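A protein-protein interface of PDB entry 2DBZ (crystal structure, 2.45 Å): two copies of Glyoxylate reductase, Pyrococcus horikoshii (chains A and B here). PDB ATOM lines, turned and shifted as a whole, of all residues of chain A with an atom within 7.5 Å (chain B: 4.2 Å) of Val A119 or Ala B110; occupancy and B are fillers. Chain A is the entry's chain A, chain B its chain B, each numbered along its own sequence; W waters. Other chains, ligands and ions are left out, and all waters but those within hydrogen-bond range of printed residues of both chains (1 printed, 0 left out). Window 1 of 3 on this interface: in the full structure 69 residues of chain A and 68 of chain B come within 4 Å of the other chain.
The backbone NH of Val A119 is in hydrogen-bond range of the backbone carbonyl oxygen of Ala A114 (3.0 Å).
Among the printed residues, merely in contact across the chains: Ala A110 with Leu B113 (3.6 Å), Leu A113 with Asp B106 (3.9 Å), Leu A113 with Ala B110 (3.5 Å), Leu A113 with Leu B113 (3.9 Å), Arg A117 with Asp B106 (3.9 Å), Arg A117 with Leu B107 (3.9 Å), Val A119 with Ala B110 (3.9 Å), Asp A123 with Val B284 (3.6 Å) and Phe A172 with Asp B106 (3.4 Å).
Printed residues of chain B within 4 Å of Leu A113: Asp B106 (3.9 Å), Ala B110 (3.5 Å) and Leu B113 (3.9 Å). Of chain B, only Ala B110 comes within 4 Å of Val A119. Printed residues of chain B within 4 Å of Phe A172: Asp B106. Printed residues of chain A within 4 Å of Leu B107: Arg A117 (3.9 Å). Ala B110 touches just these residues of chain A: Leu A113 and Val A119. Of the printed residues of chain A, Leu B113 touches Ala A110 (3.6 Å) and Leu A113 (3.9 Å). Printed residues of chain A within 4 Å of Val B284: Asp A123. The nearest printed residue of chain B that does not touch Val A119 is Thr B286 (4.04 Å). The nearest residue of chain A that does not touch Ala B110 is Ala A114 (4.6 Å). The nearest printed residue of chain B that does not touch Asp A123 is Thr B286 (4.7 Å).
Of the 20 printed residues of chain A, 6 touch a printed residue of chain B. Printed residues of chain B that touch a printed residue of chain A: Asp B106, Leu B107, Ala B110, Leu B113 and Val B284. Hydrophobic or aromatic side chains of chain B that line the printed part of chain A: Leu B107, Ala B110 and Leu B113. Among the printed residues, no Asp or Glu carboxylate lies within 4 Å of a Lys or Arg side-chain nitrogen of the other chain.
Ala A110 touches Leu B113, and with the chains exchanged Leu A113 touches Ala B110. Leu A113 touches its own counterpart, Leu B113. Positions printed for both chains: 109, 110, 111, 112, 113, 114 and 284.
Water W1 lies within hydrogen-bond range of the guanidinium group of Arg A117 (2.9 Å) and the side-chain carboxylate of Asp B106 (3.0 Å).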
ATOM      1  N   PHE A 109      12.540  17.318  25.976  1.00  0.00           N
ATOM      2  CA  PHE A 109      13.934  17.038  25.670  1.00  0.00           C
ATOM      3  C   PHE A 109      14.699  18.287  25.275  1.00  0.00           C
ATOM      4  O   PHE A 109      15.918  18.369  25.462  1.00  0.00           O
ATOM      5  CB  PHE A 109      14.054  15.971  24.589  1.00  0.00           C
ATOM      6  CG  PHE A 109      14.677  14.713  25.095  1.00  0.00           C
ATOM      7  CD1 PHE A 109      13.896  13.712  25.673  1.00  0.00           C
ATOM      8  CD2 PHE A 109      16.053  14.562  25.069  1.00  0.00           C
ATOM      9  CE1 PHE A 109      14.489  12.588  26.219  1.00  0.00           C
ATOM     10  CE2 PHE A 109      16.646  13.450  25.610  1.00  0.00           C
ATOM     11  CZ  PHE A 109      15.857  12.464  26.187  1.00  0.00           C
ATOM     12  N   ALA A 110      13.995  19.275  24.737  1.00  0.00           N
ATOM     13  CA  ALA A 110      14.690  20.497  24.378  1.00  0.00           C
ATOM     14  C   ALA A 110      15.177  21.160  25.667  1.00  0.00           C
ATOM     15  O   ALA A 110      16.288  21.686  25.701  1.00  0.00           O
ATOM     16  CB  ALA A 110      13.763  21.445  23.607  1.00  0.00           C
ATOM     17  N   LEU A 111      14.367  21.111  26.732  1.00  0.00           N
ATOM     18  CA  LEU A 111      14.761  21.752  27.999  1.00  0.00           C
ATOM     19  C   LEU A 111      15.922  21.004  28.626  1.00  0.00           C
ATOM     20  O   LEU A 111      16.908  21.602  29.099  1.00  0.00           O
ATOM     21  CB  LEU A 111      13.577  21.840  28.963  1.00  0.00           C
ATOM     22  CG  LEU A 111      12.485  22.862  28.590  1.00  0.00           C
ATOM     23  CD1 LEU A 111      11.377  22.928  29.684  1.00  0.00           C
ATOM     24  CD2 LEU A 111      13.137  24.228  28.404  1.00  0.00           C
ATOM     25  N   LEU A 112      15.808  19.683  28.592  1.00  0.00           N
ATOM     26  CA  LEU A 112      16.847  18.816  29.107  1.00  0.00           C
ATOM     27  C   LEU A 112      18.195  19.186  28.493  1.00  0.00           C
ATOM     28  O   LEU A 112      19.154  19.484  29.209  1.00  0.00           O
ATOM     29  CB  LEU A 112      16.494  17.352  28.797  1.00  0.00           C
ATOM     30  CG  LEU A 112      17.322  16.252  29.477  1.00  0.00           C
ATOM     31  CD1 LEU A 112      16.555  14.939  29.477  1.00  0.00           C
ATOM     32  CD2 LEU A 112      18.645  16.068  28.769  1.00  0.00           C
ATOM     33  N   LEU A 113      18.279  19.190  27.168  1.00  0.00           N
ATOM     34  CA  LEU A 113      19.550  19.512  26.520  1.00  0.00           C
ATOM     35  C   LEU A 113      20.018  20.965  26.696  1.00  0.00           C
ATOM     36  O   LEU A 113      21.217  21.213  26.866  1.00  0.00           O
ATOM     37  CB  LEU A 113      19.473  19.149  25.031  1.00  0.00           C
ATOM     38  CG  LEU A 113      19.360  17.639  24.789  1.00  0.00           C
ATOM     39  CD1 LEU A 113      18.716  17.371  23.429  1.00  0.00           C
ATOM     40  CD2 LEU A 113      20.745  16.995  24.875  1.00  0.00           C
ATOM     41  N   ALA A 114      19.077  21.917  26.656  1.00  0.00           N
ATOM     42  CA  ALA A 114      19.434  23.319  26.823  1.00  0.00           C
ATOM     43  C   ALA A 114      19.984  23.586  28.239  1.00  0.00           C
ATOM     44  O   ALA A 114      20.967  24.322  28.402  1.00  0.00           O
ATOM     45  CB  ALA A 114      18.240  24.209  26.544  1.00  0.00           C
ATOM     46  N   THR A 115      19.373  22.992  29.263  1.00  0.00           N
ATOM     47  CA  THR A 115      19.869  23.207  30.621  1.00  0.00           C
ATOM     48  C   THR A 115      21.239  22.522  30.803  1.00  0.00           C
ATOM     49  O   THR A 115      22.181  23.120  31.332  1.00  0.00           O
ATOM     50  CB  THR A 115      18.891  22.653  31.651  1.00  0.00           C
ATOM     51  OG1 THR A 115      17.583  23.200  31.411  1.00  0.00           O
ATOM     52  CG2 THR A 115      19.363  23.001  33.079  1.00  0.00           C
ATOM     53  N   ALA A 116      21.347  21.283  30.322  1.00  0.00           N
ATOM     54  CA  ALA A 116      22.571  20.489  30.423  1.00  0.00           C
ATOM     55  C   ALA A 116      23.768  21.115  29.732  1.00  0.00           C
ATOM     56  O   ALA A 116      24.932  20.963  30.181  1.00  0.00           O
ATOM     57  CB  ALA A 116      22.328  19.088  29.821  1.00  0.00           C
ATOM     58  N   ARG A 117      23.492  21.820  28.640  1.00  0.00           N
ATOM     59  CA  ARG A 117      24.587  22.362  27.860  1.00  0.00           C
ATOM     60  C   ARG A 117      24.703  23.862  27.799  1.00  0.00           C
ATOM     61  O   ARG A 117      25.511  24.370  27.053  1.00  0.00           O
ATOM     62  CB  ARG A 117      24.565  21.738  26.448  1.00  0.00           C
ATOM     63  CG  ARG A 117      24.745  20.207  26.494  1.00  0.00           C
ATOM     64  CD  ARG A 117      26.089  19.829  27.132  1.00  0.00           C
ATOM     65  NE  ARG A 117      27.147  20.383  26.293  1.00  0.00           N
ATOM     66  CZ  ARG A 117      27.625  19.793  25.202  1.00  0.00           C
ATOM     67  NH1 ARG A 117      27.163  18.602  24.828  1.00  0.00           N
ATOM     68  NH2 ARG A 117      28.500  20.444  24.437  1.00  0.00           N
ATOM     69  N   HIS A 118      23.930  24.556  28.620  1.00  0.00           N
ATOM     70  CA  HIS A 118      23.975  26.006  28.697  1.00  0.00           C
ATOM     71  C   HIS A 118      23.653  26.679  27.362  1.00  0.00           C
ATOM     72  O   HIS A 118      24.359  27.606  26.953  1.00  0.00           O
ATOM     73  CB  HIS A 118      25.367  26.453  29.150  1.00  0.00           C
ATOM     74  CG  HIS A 118      25.877  25.733  30.362  1.00  0.00           C
ATOM     75  ND1 HIS A 118      25.246  25.795  31.586  1.00  0.00           N
ATOM     76  CD2 HIS A 118      26.964  24.939  30.538  1.00  0.00           C
ATOM     77  CE1 HIS A 118      25.918  25.065  32.461  1.00  0.00           C
ATOM     78  NE2 HIS A 118      26.965  24.536  31.851  1.00  0.00           N
ATOM     79  N   VAL A 119      22.595  26.244  26.687  1.00  0.00           N
ATOM     80  CA  VAL A 119      22.281  26.838  25.389  1.00  0.00           C
ATOM     81  C   VAL A 119      21.835  28.300  25.484  1.00  0.00           C
ATOM     82  O   VAL A 119      22.338  29.159  24.750  1.00  0.00           O
ATOM     83  CB  VAL A 119      21.214  26.007  24.639  1.00  0.00           C
ATOM     84  CG1 VAL A 119      20.700  26.780  23.469  1.00  0.00           C
ATOM     85  CG2 VAL A 119      21.827  24.697  24.135  1.00  0.00           C
ATOM     86  N   VAL A 120      20.894  28.569  26.389  1.00  0.00           N
ATOM     87  CA  VAL A 120      20.370  29.913  26.596  1.00  0.00           C
ATOM     88  C   VAL A 120      21.480  30.880  27.022  1.00  0.00           C
ATOM     89  O   VAL A 120      21.599  32.012  26.520  1.00  0.00           O
ATOM     90  CB  VAL A 120      19.269  29.900  27.665  1.00  0.00           C
ATOM     91  CG1 VAL A 120      18.769  31.290  27.917  1.00  0.00           C
ATOM     92  CG2 VAL A 120      18.121  29.002  27.212  1.00  0.00           C
ATOM     93  N   LYS A 121      22.307  30.425  27.947  1.00  0.00           N
ATOM     94  CA  LYS A 121      23.404  31.241  28.431  1.00  0.00           C
ATOM     95  C   LYS A 121      24.394  31.520  27.302  1.00  0.00           C
ATOM     96  O   LYS A 121      24.829  32.644  27.108  1.00  0.00           O
ATOM     97  CB  LYS A 121      24.074  30.501  29.586  1.00  0.00           C
ATOM     98  CG  LYS A 121      25.293  31.153  30.219  1.00  0.00           C
ATOM     99  CD  LYS A 121      25.759  30.283  31.389  1.00  0.00           C
ATOM    100  CE  LYS A 121      27.110  30.723  31.912  1.00  0.00           C
ATOM    101  NZ  LYS A 121      27.539  29.840  33.024  1.00  0.00           N
ATOM    102  N   GLY A 122      24.740  30.484  26.549  1.00  0.00           N
ATOM    103  CA  GLY A 122      25.688  30.648  25.465  1.00  0.00           C
ATOM    104  C   GLY A 122      25.204  31.632  24.424  1.00  0.00           C
ATOM    105  O   GLY A 122      25.995  32.397  23.856  1.00  0.00           O
ATOM    106  N   ASP A 123      23.899  31.603  24.174  1.00  0.00           N
ATOM    107  CA  ASP A 123      23.283  32.483  23.185  1.00  0.00           C
ATOM    108  C   ASP A 123      23.364  33.938  23.637  1.00  0.00           C
ATOM    109  O   ASP A 123      23.748  34.811  22.858  1.00  0.00           O
ATOM    110  CB  ASP A 123      21.832  32.071  22.955  1.00  0.00           C
ATOM    111  CG  ASP A 123      21.138  32.922  21.903  1.00  0.00           C
ATOM    112  OD1 ASP A 123      20.763  34.077  22.229  1.00  0.00           O
ATOM    113  OD2 ASP A 123      20.970  32.437  20.751  1.00  0.00           O
ATOM    114  N   ARG A 124      23.000  34.189  24.891  1.00  0.00           N
ATOM    115  CA  ARG A 124      23.079  35.529  25.441  1.00  0.00           C
ATOM    116  C   ARG A 124      24.540  36.031  25.300  1.00  0.00           C
ATOM    117  O   ARG A 124      24.787  37.141  24.841  1.00  0.00           O
ATOM    118  CB  ARG A 124      22.672  35.477  26.903  1.00  0.00           C
ATOM    119  CG  ARG A 124      21.880  36.677  27.391  1.00  0.00           C
ATOM    120  CD  ARG A 124      21.460  36.443  28.835  1.00  0.00           C
ATOM    121  NE  ARG A 124      21.007  35.065  29.035  1.00  0.00           N
ATOM    122  CZ  ARG A 124      20.632  34.557  30.206  1.00  0.00           C
ATOM    123  NH1 ARG A 124      20.643  35.318  31.296  1.00  0.00           N
ATOM    124  NH2 ARG A 124      20.276  33.276  30.296  1.00  0.00           N
ATOM    125  N   PHE A 125      25.498  35.189  25.676  1.00  0.00           N
ATOM    126  CA  PHE A 125      26.917  35.506  25.591  1.00  0.00           C
ATOM    127  C   PHE A 125      27.335  35.898  24.175  1.00  0.00           C
ATOM    128  O   PHE A 125      28.085  36.874  23.980  1.00  0.00           O
ATOM    129  CB  PHE A 125      27.727  34.289  26.028  1.00  0.00           C
ATOM    130  CG  PHE A 125      29.213  34.530  26.123  1.00  0.00           C
ATOM    131  CD1 PHE A 125      29.733  35.430  27.052  1.00  0.00           C
ATOM    132  CD2 PHE A 125      30.103  33.784  25.344  1.00  0.00           C
ATOM    133  CE1 PHE A 125      31.130  35.579  27.215  1.00  0.00           C
ATOM    134  CE2 PHE A 125      31.504  33.923  25.496  1.00  0.00           C
ATOM    135  CZ  PHE A 125      32.015  34.823  26.438  1.00  0.00           C
ATOM    136  N   PHE A 143      31.961  27.025  29.277  1.00  0.00           N
ATOM    137  CA  PHE A 143      30.608  26.502  29.170  1.00  0.00           C
ATOM    138  C   PHE A 143      30.503  24.973  29.313  1.00  0.00           C
ATOM    139  O   PHE A 143      29.607  24.340  28.758  1.00  0.00           O
ATOM    140  CB  PHE A 143      30.003  26.966  27.836  1.00  0.00           C
ATOM    141  CG  PHE A 143      29.818  28.466  27.733  1.00  0.00           C
ATOM    142  CD1 PHE A 143      28.679  29.089  28.252  1.00  0.00           C
ATOM    143  CD2 PHE A 143      30.798  29.263  27.132  1.00  0.00           C
ATOM    144  CE1 PHE A 143      28.518  30.495  28.171  1.00  0.00           C
ATOM    145  CE2 PHE A 143      30.650  30.660  27.045  1.00  0.00           C
ATOM    146  CZ  PHE A 143      29.513  31.277  27.563  1.00  0.00           C
ATOM    147  N   PHE A 172      19.159   8.396  22.909  1.00  0.00           N
ATOM    148  CA  PHE A 172      20.400   8.850  23.537  1.00  0.00           C
ATOM    149  C   PHE A 172      21.033   7.746  24.383  1.00  0.00           C
ATOM    150  O   PHE A 172      21.878   8.013  25.249  1.00  0.00           O
ATOM    151  CB  PHE A 172      20.164  10.088  24.404  1.00  0.00           C
ATOM    152  CG  PHE A 172      19.903  11.338  23.616  1.00  0.00           C
ATOM    153  CD1 PHE A 172      18.677  11.552  22.999  1.00  0.00           C
ATOM    154  CD2 PHE A 172      20.894  12.300  23.483  1.00  0.00           C
ATOM    155  CE1 PHE A 172      18.449  12.713  22.262  1.00  0.00           C
ATOM    156  CE2 PHE A 172      20.670  13.464  22.747  1.00  0.00           C
ATOM    157  CZ  PHE A 172      19.450  13.674  22.137  1.00  0.00           C
ATOM    158  N   VAL A 284      16.682  27.169  32.871  1.00  0.00           N
ATOM    159  CA  VAL A 284      16.148  27.473  31.542  1.00  0.00           C
ATOM    160  C   VAL A 284      14.639  27.557  31.711  1.00  0.00           C
ATOM    161  O   VAL A 284      14.016  26.664  32.295  1.00  0.00           O
ATOM    162  CB  VAL A 284      16.509  26.372  30.490  1.00  0.00           C
ATOM    163  CG1 VAL A 284      15.803  26.640  29.163  1.00  0.00           C
ATOM    164  CG2 VAL A 284      18.004  26.355  30.262  1.00  0.00           C
ATOM    165  N   ASP B 106      25.067  15.552  20.982  1.00  0.00           N
ATOM    166  CA  ASP B 106      24.138  16.033  22.011  1.00  0.00           C
ATOM    167  C   ASP B 106      23.887  17.549  21.757  1.00  0.00           C
ATOM    168  O   ASP B 106      22.744  17.998  21.724  1.00  0.00           O
ATOM    169  CB  ASP B 106      24.723  15.835  23.425  1.00  0.00           C
ATOM    170  CG  ASP B 106      24.636  14.387  23.928  1.00  0.00           C
ATOM    171  OD1 ASP B 106      24.114  13.493  23.208  1.00  0.00           O
ATOM    172  OD2 ASP B 106      25.108  14.152  25.069  1.00  0.00           O
ATOM    173  N   LEU B 107      24.941  18.343  21.558  1.00  0.00           N
ATOM    174  CA  LEU B 107      24.722  19.765  21.312  1.00  0.00           C
ATOM    175  C   LEU B 107      23.986  20.051  19.989  1.00  0.00           C
ATOM    176  O   LEU B 107      23.153  20.978  19.922  1.00  0.00           O
ATOM    177  CB  LEU B 107      26.035  20.552  21.357  1.00  0.00           C
ATOM    178  CG  LEU B 107      25.700  22.034  21.118  1.00  0.00           C
ATOM    179  CD1 LEU B 107      25.313  22.682  22.435  1.00  0.00           C
ATOM    180  CD2 LEU B 107      26.868  22.771  20.514  1.00  0.00           C
ATOM    181  N   ALA B 108      24.266  19.270  18.945  1.00  0.00           N
ATOM    182  CA  ALA B 108      23.570  19.488  17.664  1.00  0.00           C
ATOM    183  C   ALA B 108      22.068  19.329  17.891  1.00  0.00           C
ATOM    184  O   ALA B 108      21.264  20.141  17.407  1.00  0.00           O
ATOM    185  CB  ALA B 108      24.033  18.493  16.605  1.00  0.00           C
ATOM    186  N   PHE B 109      21.676  18.296  18.637  1.00  0.00           N
ATOM    187  CA  PHE B 109      20.250  18.127  18.873  1.00  0.00           C
ATOM    188  C   PHE B 109      19.682  19.198  19.789  1.00  0.00           C
ATOM    189  O   PHE B 109      18.522  19.579  19.664  1.00  0.00           O
ATOM    190  CB  PHE B 109      19.949  16.734  19.416  1.00  0.00           C
ATOM    191  CG  PHE B 109      19.201  15.887  18.443  1.00  0.00           C
ATOM    192  CD1 PHE B 109      19.875  15.186  17.449  1.00  0.00           C
ATOM    193  CD2 PHE B 109      17.817  15.847  18.476  1.00  0.00           C
ATOM    194  CE1 PHE B 109      19.171  14.460  16.496  1.00  0.00           C
ATOM    195  CE2 PHE B 109      17.110  15.129  17.530  1.00  0.00           C
ATOM    196  CZ  PHE B 109      17.798  14.437  16.539  1.00  0.00           C
ATOM    197  N   ALA B 110      20.489  19.693  20.720  1.00  0.00           N
ATOM    198  CA  ALA B 110      19.993  20.753  21.574  1.00  0.00           C
ATOM    199  C   ALA B 110      19.650  21.948  20.673  1.00  0.00           C
ATOM    200  O   ALA B 110      18.609  22.577  20.845  1.00  0.00           O
ATOM    201  CB  ALA B 110      21.045  21.147  22.603  1.00  0.00           C
ATOM    202  N   LEU B 111      20.513  22.238  19.697  1.00  0.00           N
ATOM    203  CA  LEU B 111      20.293  23.377  18.785  1.00  0.00           C
ATOM    204  C   LEU B 111      19.069  23.178  17.906  1.00  0.00           C
ATOM    205  O   LEU B 111      18.243  24.092  17.717  1.00  0.00           O
ATOM    206  CB  LEU B 111      21.534  23.632  17.913  1.00  0.00           C
ATOM    207  CG  LEU B 111      22.736  24.244  18.642  1.00  0.00           C
ATOM    208  CD1 LEU B 111      23.911  24.528  17.657  1.00  0.00           C
ATOM    209  CD2 LEU B 111      22.281  25.542  19.302  1.00  0.00           C
ATOM    210  N   LEU B 112      18.968  21.973  17.367  1.00  0.00           N
ATOM    211  CA  LEU B 112      17.833  21.607  16.547  1.00  0.00           C
ATOM    212  C   LEU B 112      16.550  21.865  17.341  1.00  0.00           C
ATOM    213  O   LEU B 112      15.641  22.549  16.868  1.00  0.00           O
ATOM    214  CB  LEU B 112      17.955  20.122  16.161  1.00  0.00           C
ATOM    215  CG  LEU B 112      16.966  19.534  15.151  1.00  0.00           C
ATOM    216  CD1 LEU B 112      17.583  18.309  14.494  1.00  0.00           C
ATOM    217  CD2 LEU B 112      15.633  19.202  15.841  1.00  0.00           C
ATOM    218  N   LEU B 113      16.481  21.340  18.559  1.00  0.00           N
ATOM    219  CA  LEU B 113      15.277  21.518  19.356  1.00  0.00           C
ATOM    220  C   LEU B 113      15.038  22.942  19.848  1.00  0.00           C
ATOM    221  O   LEU B 113      13.902  23.412  19.874  1.00  0.00           O
ATOM    222  CB  LEU B 113      15.281  20.529  20.525  1.00  0.00           C
ATOM    223  CG  LEU B 113      15.054  19.072  20.081  1.00  0.00           C
ATOM    224  CD1 LEU B 113      15.602  18.125  21.166  1.00  0.00           C
ATOM    225  CD2 LEU B 113      13.555  18.820  19.779  1.00  0.00           C
ATOM    226  N   ALA B 114      16.107  23.624  20.242  1.00  0.00           N
ATOM    227  CA  ALA B 114      15.985  24.993  20.716  1.00  0.00           C
ATOM    228  C   ALA B 114      15.446  25.912  19.609  1.00  0.00           C
ATOM    229  O   ALA B 114      14.582  26.750  19.860  1.00  0.00           O
ATOM    230  CB  ALA B 114      17.330  25.491  21.194  1.00  0.00           C
ATOM    231  N   VAL B 284      19.474  30.664  16.795  1.00  0.00           N
ATOM    232  CA  VAL B 284      19.935  30.275  18.124  1.00  0.00           C
ATOM    233  C   VAL B 284      21.427  30.153  17.917  1.00  0.00           C
ATOM    234  O   VAL B 284      21.865  29.530  16.941  1.00  0.00           O
ATOM    235  CB  VAL B 284      19.334  28.901  18.560  1.00  0.00           C
ATOM    236  CG1 VAL B 284      20.026  28.370  19.816  1.00  0.00           C
ATOM    237  CG2 VAL B 284      17.838  29.056  18.814  1.00  0.00           C
ATOM    238  N   THR B 286      25.510  29.600  19.793  1.00  0.00           N
ATOM    239  CA  THR B 286      26.297  29.149  20.923  1.00  0.00           C
ATOM    240  C   THR B 286      27.713  29.357  20.492  1.00  0.00           C
ATOM    241  O   THR B 286      28.025  29.196  19.313  1.00  0.00           O
ATOM    242  CB  THR B 286      26.045  27.678  21.275  1.00  0.00           C
ATOM    243  OG1 THR B 286      26.174  26.860  20.104  1.00  0.00           O
ATOM    244  CG2 THR B 286      24.658  27.539  21.868  1.00  0.00           C
HETATM  245  O   HOH W   1      25.953  16.619  26.485  1.00  0.00           O
